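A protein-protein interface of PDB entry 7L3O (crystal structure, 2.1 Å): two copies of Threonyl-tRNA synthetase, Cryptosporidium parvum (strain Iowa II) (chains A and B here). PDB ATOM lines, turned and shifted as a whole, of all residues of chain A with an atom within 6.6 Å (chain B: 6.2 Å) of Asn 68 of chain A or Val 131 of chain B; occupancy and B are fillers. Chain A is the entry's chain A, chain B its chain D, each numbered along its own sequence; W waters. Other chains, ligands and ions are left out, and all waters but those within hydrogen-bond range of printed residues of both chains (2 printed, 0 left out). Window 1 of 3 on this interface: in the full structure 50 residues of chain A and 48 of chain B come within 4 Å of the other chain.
The guanidinium group (NE) of Arg 149 of chain B sits at hydrogen-bond distance from the side-chain amide oxygen (OD1) of Asn 68 of chain A, 3.3 Å away. The backbone carbonyl oxygen (O) of Ile 69 of chain A sits at hydrogen-bond distance from the side-chain hydroxyl (OG) of Ser 31 of chain B, 2.8 Å away. NE of Arg 149 of chain A sits at hydrogen-bond distance from OD1 of Asn 68 of chain B (3.2 Å).
The backbone carbonyl oxygen (O) of Pro 67 of chain A is in hydrogen-bond range of the side-chain amino group (NZ) of Lys 101 of chain A (3.1 Å). O of Asn 68 of chain A is in hydrogen-bond range of N of Lys 101 of chain A, at 2.8 Å. ND2 of Asn 68 of chain A lies within hydrogen-bond range of O of Val 131 of chain A, at 3.2 Å. The backbone carbonyl oxygen (O) of Lys 101 of chain A is in hydrogen-bond range of the backbone NH (N) of His 133 of chain A (3.0 Å). O of Lys 101 of chain B lies within hydrogen-bond range of N of His 133 of chain B, 3.0 Å away. OE1 of Gln 151 of chain B sits at hydrogen-bond distance from NH1 of Arg 149 of chain B.
Among the printed residues, merely in contact across the chains: Pro 67 of chain A with Ser 31 of chain B, Val 131 of chain A with Asn 68 of chain B, Asn 68 of chain A with Val 131 of chain B, Pro 67 of chain A with Ser 34 of chain B, His 133 of chain A with Asn 68 of chain B, Asn 68 of chain A with His 133 of chain B, Phe 70 of chain A with Ser 31 of chain B, Ile 69 of chain A with Leu 100 of chain B and Ile 69 of chain A with His 133 of chain B.
Of chain B, only Val 131, His 133 and Arg 149 come within 4 Å of Asn 68 of chain A. Trp 75 of chain A touches none of the printed residues of chain B. Of the printed residues of chain B, His 133 of chain A touches Asn 68 (3.6 Å). Printed residues of chain B within 4 Å of Arg 149 of chain A: Asn 68 (3.2 Å). Of the printed residues of chain A, Leu 100 of chain B touches Ile 69 (3.8 Å). Val 131 of chain B touches just one residue of chain A: Asn 68 (3.4 Å). The nearest printed residue of chain B that does not touch Phe 70 of chain A is Ser 34 of chain B (6.7 Å).
Printed residues of chain B that touch a printed residue of chain A: Ser 31, Ser 34, Asn 68, Leu 100, Val 131, His 133 and Arg 149. Hydrophobic or aromatic side chains of chain B that line the printed part of chain A: Leu 100, Val 131 and His 133. Hydrophobic or aromatic side chains of chain A that line the printed part of chain B: Pro 67, Ile 69, Phe 70, Val 131 and His 133. Among the printed residues, 12 pairs touch across the chains. Among the printed residues, no Asp or Glu carboxylate lies within 4 Å of a Lys or Arg side-chain nitrogen of the other chain.
Asn 68 of chain A touches Val 131 of chain B, and with the chains exchanged Val 131 of chain A touches Asn 68 of chain B. Asn 68 of chain A touches His 133 of chain B, and with the chains exchanged His 133 of chain A touches Asn 68 of chain B. Asn 68 of chain A touches Arg 149 of chain B, and with the chains exchanged Arg 149 of chain A touches Asn 68 of chain B. Of the 12 pairs that touch across the chains among the printed residues, 6 have their exchanged pair printed and touching as well.
Water W2 lies within hydrogen-bond range of NE2 of His 133 of chain A (2.6 Å) and N of Asn 68 of chain B (2.8 Å). Water W1 lies within hydrogen-bond range of the backbone NH (N) of Asn 68 of chain A (2.7 Å), a ring nitrogen (NE2) of His 133 of chain B (2.8 Å), the side-chain hydroxyl (OG) of Ser 34 of chain B (3.0 Å) and the backbone NH (N) of Ile 69 of chain A (3.1 Å).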
ATOM      1  N   THR A  66     -15.465 -18.296 -29.488  1.00  0.00           N
ATOM      2  CA  THR A  66     -16.238 -17.925 -30.663  1.00  0.00           C
ATOM      3  C   THR A  66     -17.725 -17.953 -30.333  1.00  0.00           C
ATOM      4  O   THR A  66     -18.131 -18.522 -29.317  1.00  0.00           O
ATOM      5  CB  THR A  66     -15.938 -18.871 -31.844  1.00  0.00           C
ATOM      6  OG1 THR A  66     -16.147 -20.228 -31.442  1.00  0.00           O
ATOM      7  CG2 THR A  66     -14.495 -18.733 -32.248  1.00  0.00           C
ATOM      8  N   PRO A  67     -18.561 -17.318 -31.156  1.00  0.00           N
ATOM      9  CA  PRO A  67     -20.014 -17.390 -30.959  1.00  0.00           C
ATOM     10  C   PRO A  67     -20.527 -18.818 -30.999  1.00  0.00           C
ATOM     11  O   PRO A  67     -19.855 -19.757 -31.431  1.00  0.00           O
ATOM     12  CB  PRO A  67     -20.571 -16.589 -32.139  1.00  0.00           C
ATOM     13  CG  PRO A  67     -19.482 -15.615 -32.473  1.00  0.00           C
ATOM     14  CD  PRO A  67     -18.191 -16.343 -32.196  1.00  0.00           C
ATOM     15  N   ASN A  68     -21.764 -18.970 -30.539  1.00  0.00           N
ATOM     16  CA  ASN A  68     -22.477 -20.230 -30.664  1.00  0.00           C
ATOM     17  C   ASN A  68     -23.525 -20.205 -31.755  1.00  0.00           C
ATOM     18  O   ASN A  68     -23.869 -21.265 -32.282  1.00  0.00           O
ATOM     19  CB  ASN A  68     -23.160 -20.590 -29.349  1.00  0.00           C
ATOM     20  CG  ASN A  68     -22.172 -20.776 -28.231  1.00  0.00           C
ATOM     21  OD1 ASN A  68     -21.862 -19.832 -27.520  1.00  0.00           O
ATOM     22  ND2 ASN A  68     -21.660 -21.996 -28.074  1.00  0.00           N
ATOM     23  N   ILE A  69     -24.055 -19.028 -32.083  1.00  0.00           N
ATOM     24  CA  ILE A  69     -25.061 -18.879 -33.125  1.00  0.00           C
ATOM     25  C   ILE A  69     -24.484 -18.004 -34.222  1.00  0.00           C
ATOM     26  O   ILE A  69     -23.709 -17.073 -33.961  1.00  0.00           O
ATOM     27  CB  ILE A  69     -26.384 -18.281 -32.605  1.00  0.00           C
ATOM     28  CG1 ILE A  69     -26.174 -16.867 -32.048  1.00  0.00           C
ATOM     29  CG2 ILE A  69     -27.020 -19.174 -31.543  1.00  0.00           C
ATOM     30  CD1 ILE A  69     -27.497 -16.174 -31.750  1.00  0.00           C
ATOM     31  N   PHE A  70     -24.875 -18.312 -35.461  1.00  0.00           N
ATOM     32  CA  PHE A  70     -24.371 -17.640 -36.650  1.00  0.00           C
ATOM     33  C   PHE A  70     -25.461 -17.564 -37.712  1.00  0.00           C
ATOM     34  O   PHE A  70     -26.339 -18.430 -37.789  1.00  0.00           O
ATOM     35  CB  PHE A  70     -23.168 -18.369 -37.262  1.00  0.00           C
ATOM     36  CG  PHE A  70     -22.014 -18.544 -36.326  1.00  0.00           C
ATOM     37  CD1 PHE A  70     -21.976 -19.607 -35.437  1.00  0.00           C
ATOM     38  CD2 PHE A  70     -20.951 -17.657 -36.349  1.00  0.00           C
ATOM     39  CE1 PHE A  70     -20.893 -19.773 -34.573  1.00  0.00           C
ATOM     40  CE2 PHE A  70     -19.868 -17.823 -35.497  1.00  0.00           C
ATOM     41  CZ  PHE A  70     -19.842 -18.881 -34.605  1.00  0.00           C
ATOM     42  N   TRP A  75     -22.187 -20.996 -43.045  1.00  0.00           N
ATOM     43  CA  TRP A  75     -22.053 -22.387 -43.440  1.00  0.00           C
ATOM     44  C   TRP A  75     -22.275 -22.579 -44.922  1.00  0.00           C
ATOM     45  O   TRP A  75     -21.805 -23.581 -45.471  1.00  0.00           O
ATOM     46  CB  TRP A  75     -22.994 -23.246 -42.616  1.00  0.00           C
ATOM     47  CG  TRP A  75     -22.598 -23.108 -41.204  1.00  0.00           C
ATOM     48  CD1 TRP A  75     -21.362 -23.355 -40.681  1.00  0.00           C
ATOM     49  CD2 TRP A  75     -23.403 -22.641 -40.134  1.00  0.00           C
ATOM     50  NE1 TRP A  75     -21.350 -23.090 -39.344  1.00  0.00           N
ATOM     51  CE2 TRP A  75     -22.591 -22.649 -38.975  1.00  0.00           C
ATOM     52  CE3 TRP A  75     -24.732 -22.218 -40.035  1.00  0.00           C
ATOM     53  CZ2 TRP A  75     -23.066 -22.261 -37.723  1.00  0.00           C
ATOM     54  CZ3 TRP A  75     -25.209 -21.836 -38.800  1.00  0.00           C
ATOM     55  CH2 TRP A  75     -24.373 -21.855 -37.653  1.00  0.00           C
ATOM     56  N   GLY A  99     -28.322 -20.477 -37.246  1.00  0.00           N
ATOM     57  CA  GLY A  99     -28.249 -21.769 -36.594  1.00  0.00           C
ATOM     58  C   GLY A  99     -27.235 -21.822 -35.475  1.00  0.00           C
ATOM     59  O   GLY A  99     -26.330 -20.984 -35.371  1.00  0.00           O
ATOM     60  N   LEU A 100     -27.415 -22.828 -34.619  1.00  0.00           N
ATOM     61  CA  LEU A 100     -26.450 -23.159 -33.580  1.00  0.00           C
ATOM     62  C   LEU A 100     -25.296 -23.925 -34.198  1.00  0.00           C
ATOM     63  O   LEU A 100     -25.511 -24.824 -35.013  1.00  0.00           O
ATOM     64  CB  LEU A 100     -27.107 -24.009 -32.498  1.00  0.00           C
ATOM     65  CG  LEU A 100     -27.650 -23.364 -31.236  1.00  0.00           C
ATOM     66  CD1 LEU A 100     -28.381 -24.429 -30.415  1.00  0.00           C
ATOM     67  CD2 LEU A 100     -26.518 -22.730 -30.416  1.00  0.00           C
ATOM     68  N   LYS A 101     -24.067 -23.568 -33.827  1.00  0.00           N
ATOM     69  CA  LYS A 101     -22.928 -24.179 -34.502  1.00  0.00           C
ATOM     70  C   LYS A 101     -22.833 -25.662 -34.145  1.00  0.00           C
ATOM     71  O   LYS A 101     -23.024 -26.035 -32.982  1.00  0.00           O
ATOM     72  CB  LYS A 101     -21.618 -23.470 -34.149  1.00  0.00           C
ATOM     73  CG  LYS A 101     -21.262 -23.466 -32.673  1.00  0.00           C
ATOM     74  CD  LYS A 101     -19.841 -22.987 -32.466  1.00  0.00           C
ATOM     75  CE  LYS A 101     -19.479 -22.940 -30.982  1.00  0.00           C
ATOM     76  NZ  LYS A 101     -18.139 -22.323 -30.845  1.00  0.00           N
ATOM     77  N   PRO A 102     -22.604 -26.540 -35.139  1.00  0.00           N
ATOM     78  CA  PRO A 102     -22.275 -27.935 -34.838  1.00  0.00           C
ATOM     79  C   PRO A 102     -20.786 -28.211 -34.992  1.00  0.00           C
ATOM     80  O   PRO A 102     -20.333 -29.319 -34.694  1.00  0.00           O
ATOM     81  CB  PRO A 102     -23.116 -28.720 -35.861  1.00  0.00           C
ATOM     82  CG  PRO A 102     -23.247 -27.785 -37.026  1.00  0.00           C
ATOM     83  CD  PRO A 102     -22.945 -26.362 -36.559  1.00  0.00           C
ATOM     84  N   GLY A 130     -15.640 -24.572 -27.232  1.00  0.00           N
ATOM     85  CA  GLY A 130     -16.995 -24.069 -27.275  1.00  0.00           C
ATOM     86  C   GLY A 130     -18.026 -25.173 -27.392  1.00  0.00           C
ATOM     87  O   GLY A 130     -17.759 -26.273 -27.868  1.00  0.00           O
ATOM     88  N   VAL A 131     -19.227 -24.861 -26.927  1.00  0.00           N
ATOM     89  CA  VAL A 131     -20.316 -25.825 -26.920  1.00  0.00           C
ATOM     90  C   VAL A 131     -20.856 -25.983 -28.337  1.00  0.00           C
ATOM     91  O   VAL A 131     -21.240 -24.991 -28.978  1.00  0.00           O
ATOM     92  CB  VAL A 131     -21.421 -25.378 -25.952  1.00  0.00           C
ATOM     93  CG1 VAL A 131     -22.522 -26.439 -25.894  1.00  0.00           C
ATOM     94  CG2 VAL A 131     -20.827 -25.098 -24.564  1.00  0.00           C
ATOM     95  N   LEU A 132     -20.878 -27.228 -28.823  1.00  0.00           N
ATOM     96  CA  LEU A 132     -21.400 -27.598 -30.136  1.00  0.00           C
ATOM     97  C   LEU A 132     -22.716 -28.358 -29.987  1.00  0.00           C
ATOM     98  O   LEU A 132     -22.928 -29.078 -29.008  1.00  0.00           O
ATOM     99  CB  LEU A 132     -20.399 -28.468 -30.909  1.00  0.00           C
ATOM    100  CG  LEU A 132     -18.962 -27.948 -30.937  1.00  0.00           C
ATOM    101  CD1 LEU A 132     -18.040 -28.930 -31.644  1.00  0.00           C
ATOM    102  CD2 LEU A 132     -18.903 -26.580 -31.603  1.00  0.00           C
ATOM    103  N   HIS A 133     -23.612 -28.171 -30.958  1.00  0.00           N
ATOM    104  CA  HIS A 133     -24.928 -28.796 -30.939  1.00  0.00           C
ATOM    105  C   HIS A 133     -25.194 -29.459 -32.280  1.00  0.00           C
ATOM    106  O   HIS A 133     -25.015 -28.830 -33.330  1.00  0.00           O
ATOM    107  CB  HIS A 133     -26.050 -27.795 -30.649  1.00  0.00           C
ATOM    108  CG  HIS A 133     -26.154 -27.387 -29.213  1.00  0.00           C
ATOM    109  ND1 HIS A 133     -25.531 -26.266 -28.712  1.00  0.00           N
ATOM    110  CD2 HIS A 133     -26.847 -27.926 -28.180  1.00  0.00           C
ATOM    111  CE1 HIS A 133     -25.812 -26.149 -27.424  1.00  0.00           C
ATOM    112  NE2 HIS A 133     -26.606 -27.146 -27.077  1.00  0.00           N
ATOM    113  N   ARG A 149     -25.624 -32.179 -27.374  1.00  0.00           N
ATOM    114  CA  ARG A 149     -24.784 -31.124 -26.825  1.00  0.00           C
ATOM    115  C   ARG A 149     -23.442 -31.718 -26.432  1.00  0.00           C
ATOM    116  O   ARG A 149     -23.399 -32.720 -25.707  1.00  0.00           O
ATOM    117  CB  ARG A 149     -25.450 -30.502 -25.603  1.00  0.00           C
ATOM    118  CG  ARG A 149     -24.747 -29.261 -25.072  1.00  0.00           C
ATOM    119  CD  ARG A 149     -23.772 -29.559 -23.944  1.00  0.00           C
ATOM    120  NE  ARG A 149     -23.437 -28.319 -23.243  1.00  0.00           N
ATOM    121  CZ  ARG A 149     -22.315 -28.107 -22.568  1.00  0.00           C
ATOM    122  NH1 ARG A 149     -21.399 -29.054 -22.427  1.00  0.00           N
ATOM    123  NH2 ARG A 149     -22.102 -26.910 -22.028  1.00  0.00           N
ATOM    124  N   SER B  31     -22.114 -13.007 -37.256  1.00  0.00           N
ATOM    125  CA  SER B  31     -22.689 -13.211 -35.930  1.00  0.00           C
ATOM    126  C   SER B  31     -22.802 -11.899 -35.153  1.00  0.00           C
ATOM    127  O   SER B  31     -22.170 -11.748 -34.092  1.00  0.00           O
ATOM    128  CB  SER B  31     -21.860 -14.238 -35.156  1.00  0.00           C
ATOM    129  OG  SER B  31     -22.479 -14.605 -33.937  1.00  0.00           O
ATOM    130  N   SER B  34     -22.615 -11.348 -30.934  1.00  0.00           N
ATOM    131  CA  SER B  34     -21.736 -12.262 -30.235  1.00  0.00           C
ATOM    132  C   SER B  34     -20.305 -11.825 -30.490  1.00  0.00           C
ATOM    133  O   SER B  34     -20.029 -11.075 -31.429  1.00  0.00           O
ATOM    134  CB  SER B  34     -21.949 -13.711 -30.692  1.00  0.00           C
ATOM    135  OG  SER B  34     -23.304 -14.071 -30.540  1.00  0.00           O
ATOM    136  N   PRO B  67     -27.591 -27.900 -19.429  1.00  0.00           N
ATOM    137  CA  PRO B  67     -27.753 -27.841 -20.884  1.00  0.00           C
ATOM    138  C   PRO B  67     -27.913 -26.409 -21.365  1.00  0.00           C
ATOM    139  O   PRO B  67     -28.138 -25.474 -20.588  1.00  0.00           O
ATOM    140  CB  PRO B  67     -29.019 -28.666 -21.130  1.00  0.00           C
ATOM    141  CG  PRO B  67     -29.026 -29.645 -19.998  1.00  0.00           C
ATOM    142  CD  PRO B  67     -28.512 -28.872 -18.811  1.00  0.00           C
ATOM    143  N   ASN B  68     -27.775 -26.243 -22.681  1.00  0.00           N
ATOM    144  CA  ASN B  68     -28.018 -24.947 -23.305  1.00  0.00           C
ATOM    145  C   ASN B  68     -29.386 -24.841 -23.952  1.00  0.00           C
ATOM    146  O   ASN B  68     -29.951 -23.746 -23.975  1.00  0.00           O
ATOM    147  CB  ASN B  68     -26.947 -24.644 -24.359  1.00  0.00           C
ATOM    148  CG  ASN B  68     -25.572 -24.464 -23.755  1.00  0.00           C
ATOM    149  OD1 ASN B  68     -24.786 -25.414 -23.672  1.00  0.00           O
ATOM    150  ND2 ASN B  68     -25.276 -23.240 -23.307  1.00  0.00           N
ATOM    151  N   LEU B 100     -33.149 -21.820 -26.778  1.00  0.00           N
ATOM    152  CA  LEU B 100     -31.867 -21.583 -26.136  1.00  0.00           C
ATOM    153  C   LEU B 100     -32.060 -20.846 -24.813  1.00  0.00           C
ATOM    154  O   LEU B 100     -32.852 -19.906 -24.725  1.00  0.00           O
ATOM    155  CB  LEU B 100     -30.990 -20.733 -27.042  1.00  0.00           C
ATOM    156  CG  LEU B 100     -29.910 -21.372 -27.887  1.00  0.00           C
ATOM    157  CD1 LEU B 100     -29.251 -20.233 -28.654  1.00  0.00           C
ATOM    158  CD2 LEU B 100     -28.927 -22.095 -26.996  1.00  0.00           C
ATOM    159  N   LYS B 101     -31.320 -21.249 -23.792  1.00  0.00           N
ATOM    160  CA  LYS B 101     -31.576 -20.690 -22.465  1.00  0.00           C
ATOM    161  C   LYS B 101     -31.178 -19.219 -22.417  1.00  0.00           C
ATOM    162  O   LYS B 101     -30.086 -18.857 -22.873  1.00  0.00           O
ATOM    163  CB  LYS B 101     -30.844 -21.478 -21.379  1.00  0.00           C
ATOM    164  CG  LYS B 101     -29.331 -21.520 -21.473  1.00  0.00           C
ATOM    165  CD  LYS B 101     -28.765 -22.205 -20.235  1.00  0.00           C
ATOM    166  CE  LYS B 101     -27.255 -22.386 -20.295  1.00  0.00           C
ATOM    167  NZ  LYS B 101     -26.807 -23.138 -19.084  1.00  0.00           N
ATOM    168  N   ASN B 104     -30.133 -19.349 -16.321  1.00  0.00           N
ATOM    169  CA  ASN B 104     -29.809 -20.655 -15.755  1.00  0.00           C
ATOM    170  C   ASN B 104     -30.791 -21.156 -14.705  1.00  0.00           C
ATOM    171  O   ASN B 104     -30.801 -22.364 -14.439  1.00  0.00           O
ATOM    172  CB  ASN B 104     -28.430 -20.630 -15.085  1.00  0.00           C
ATOM    173  CG  ASN B 104     -27.312 -20.435 -16.061  1.00  0.00           C
ATOM    174  OD1 ASN B 104     -27.205 -21.153 -17.058  1.00  0.00           O
ATOM    175  ND2 ASN B 104     -26.469 -19.439 -15.793  1.00  0.00           N
ATOM    176  N   ASP B 128     -22.881 -21.601 -12.024  1.00  0.00           N
ATOM    177  CA  ASP B 128     -23.005 -21.993 -13.426  1.00  0.00           C
ATOM    178  C   ASP B 128     -22.536 -20.827 -14.278  1.00  0.00           C
ATOM    179  O   ASP B 128     -23.117 -19.742 -14.212  1.00  0.00           O
ATOM    180  CB  ASP B 128     -24.455 -22.348 -13.755  1.00  0.00           C
ATOM    181  CG  ASP B 128     -24.601 -23.165 -15.026  1.00  0.00           C
ATOM    182  OD1 ASP B 128     -23.791 -22.989 -15.965  1.00  0.00           O
ATOM    183  OD2 ASP B 128     -25.551 -23.977 -15.089  1.00  0.00           O
ATOM    184  N   PHE B 129     -21.480 -21.054 -15.055  1.00  0.00           N
ATOM    185  CA  PHE B 129     -20.970 -20.101 -16.025  1.00  0.00           C
ATOM    186  C   PHE B 129     -21.519 -20.358 -17.423  1.00  0.00           C
ATOM    187  O   PHE B 129     -20.857 -20.031 -18.408  1.00  0.00           O
ATOM    188  CB  PHE B 129     -19.446 -20.155 -16.063  1.00  0.00           C
ATOM    189  CG  PHE B 129     -18.764 -19.552 -14.858  1.00  0.00           C
ATOM    190  CD1 PHE B 129     -18.614 -18.184 -14.744  1.00  0.00           C
ATOM    191  CD2 PHE B 129     -18.228 -20.360 -13.877  1.00  0.00           C
ATOM    192  CE1 PHE B 129     -17.960 -17.624 -13.664  1.00  0.00           C
ATOM    193  CE2 PHE B 129     -17.582 -19.808 -12.780  1.00  0.00           C
ATOM    194  CZ  PHE B 129     -17.446 -18.437 -12.678  1.00  0.00           C
ATOM    195  N   GLY B 130     -22.713 -20.934 -17.532  1.00  0.00           N
ATOM    196  CA  GLY B 130     -23.194 -21.394 -18.827  1.00  0.00           C
ATOM    197  C   GLY B 130     -23.469 -20.264 -19.801  1.00  0.00           C
ATOM    198  O   GLY B 130     -23.871 -19.163 -19.427  1.00  0.00           O
ATOM    199  N   VAL B 131     -23.247 -20.550 -21.086  1.00  0.00           N
ATOM    200  CA  VAL B 131     -23.501 -19.571 -22.138  1.00  0.00           C
ATOM    201  C   VAL B 131     -24.991 -19.285 -22.240  1.00  0.00           C
ATOM    202  O   VAL B 131     -25.807 -20.199 -22.399  1.00  0.00           O
ATOM    203  CB  VAL B 131     -22.954 -20.073 -23.480  1.00  0.00           C
ATOM    204  CG1 VAL B 131     -23.203 -19.028 -24.550  1.00  0.00           C
ATOM    205  CG2 VAL B 131     -21.489 -20.366 -23.346  1.00  0.00           C
ATOM    206  N   LEU B 132     -25.353 -18.007 -22.171  1.00  0.00           N
ATOM    207  CA  LEU B 132     -26.739 -17.582 -22.271  1.00  0.00           C
ATOM    208  C   LEU B 132     -26.956 -16.809 -23.565  1.00  0.00           C
ATOM    209  O   LEU B 132     -26.048 -16.138 -24.059  1.00  0.00           O
ATOM    210  CB  LEU B 132     -27.130 -16.705 -21.065  1.00  0.00           C
ATOM    211  CG  LEU B 132     -26.822 -17.335 -19.697  1.00  0.00           C
ATOM    212  CD1 LEU B 132     -27.084 -16.350 -18.555  1.00  0.00           C
ATOM    213  CD2 LEU B 132     -27.612 -18.640 -19.487  1.00  0.00           C
ATOM    214  N   HIS B 133     -28.180 -16.865 -24.088  1.00  0.00           N
ATOM    215  CA  HIS B 133     -28.533 -16.126 -25.297  1.00  0.00           C
ATOM    216  C   HIS B 133     -29.832 -15.358 -25.128  1.00  0.00           C
ATOM    217  O   HIS B 133     -30.814 -15.888 -24.596  1.00  0.00           O
ATOM    218  CB  HIS B 133     -28.660 -17.054 -26.506  1.00  0.00           C
ATOM    219  CG  HIS B 133     -27.343 -17.512 -27.037  1.00  0.00           C
ATOM    220  ND1 HIS B 133     -26.642 -18.558 -26.480  1.00  0.00           N
ATOM    221  CD2 HIS B 133     -26.585 -17.050 -28.060  1.00  0.00           C
ATOM    222  CE1 HIS B 133     -25.516 -18.736 -27.148  1.00  0.00           C
ATOM    223  NE2 HIS B 133     -25.456 -17.834 -28.112  1.00  0.00           N
ATOM    224  N   ARG B 149     -25.041 -12.882 -26.685  1.00  0.00           N
ATOM    225  CA  ARG B 149     -24.387 -14.044 -26.092  1.00  0.00           C
ATOM    226  C   ARG B 149     -23.573 -13.565 -24.903  1.00  0.00           C
ATOM    227  O   ARG B 149     -22.713 -12.697 -25.055  1.00  0.00           O
ATOM    228  CB  ARG B 149     -23.476 -14.742 -27.117  1.00  0.00           C
ATOM    229  CG  ARG B 149     -22.844 -16.052 -26.673  1.00  0.00           C
ATOM    230  CD  ARG B 149     -21.444 -15.862 -26.077  1.00  0.00           C
ATOM    231  NE  ARG B 149     -20.709 -17.125 -26.033  1.00  0.00           N
ATOM    232  CZ  ARG B 149     -19.777 -17.417 -25.135  1.00  0.00           C
ATOM    233  NH1 ARG B 149     -19.453 -16.570 -24.181  1.00  0.00           N
ATOM    234  NH2 ARG B 149     -19.187 -18.611 -25.175  1.00  0.00           N
ATOM    235  N   PHE B 150     -23.828 -14.138 -23.732  1.00  0.00           N
ATOM    236  CA  PHE B 150     -23.045 -13.784 -22.558  1.00  0.00           C
ATOM    237  C   PHE B 150     -22.989 -14.975 -21.606  1.00  0.00           C
ATOM    238  O   PHE B 150     -23.863 -15.841 -21.622  1.00  0.00           O
ATOM    239  CB  PHE B 150     -23.622 -12.531 -21.864  1.00  0.00           C
ATOM    240  CG  PHE B 150     -25.075 -12.651 -21.510  1.00  0.00           C
ATOM    241  CD1 PHE B 150     -26.056 -12.597 -22.495  1.00  0.00           C
ATOM    242  CD2 PHE B 150     -25.467 -12.801 -20.195  1.00  0.00           C
ATOM    243  CE1 PHE B 150     -27.407 -12.730 -22.169  1.00  0.00           C
ATOM    244  CE2 PHE B 150     -26.808 -12.933 -19.863  1.00  0.00           C
ATOM    245  CZ  PHE B 150     -27.777 -12.892 -20.847  1.00  0.00           C
ATOM    246  N   GLN B 151     -21.915 -15.030 -20.820  1.00  0.00           N
ATOM    247  CA  GLN B 151     -21.797 -15.910 -19.665  1.00  0.00           C
ATOM    248  C   GLN B 151     -21.817 -15.069 -18.389  1.00  0.00           C
ATOM    249  O   GLN B 151     -21.177 -14.013 -18.322  1.00  0.00           O
ATOM    250  CB  GLN B 151     -20.502 -16.727 -19.717  1.00  0.00           C
ATOM    251  CG  GLN B 151     -20.462 -17.780 -20.835  1.00  0.00           C
ATOM    252  CD  GLN B 151     -19.090 -18.382 -21.026  1.00  0.00           C
ATOM    253  OE1 GLN B 151     -18.498 -18.295 -22.113  1.00  0.00           O
ATOM    254  NE2 GLN B 151     -18.573 -19.005 -19.977  1.00  0.00           N
HETATM  255  O   HOH W   1     -23.472 -16.997 -29.883  1.00  0.00           O
HETATM  256  O   HOH W   2     -27.563 -28.061 -24.815  1.00  0.00           O
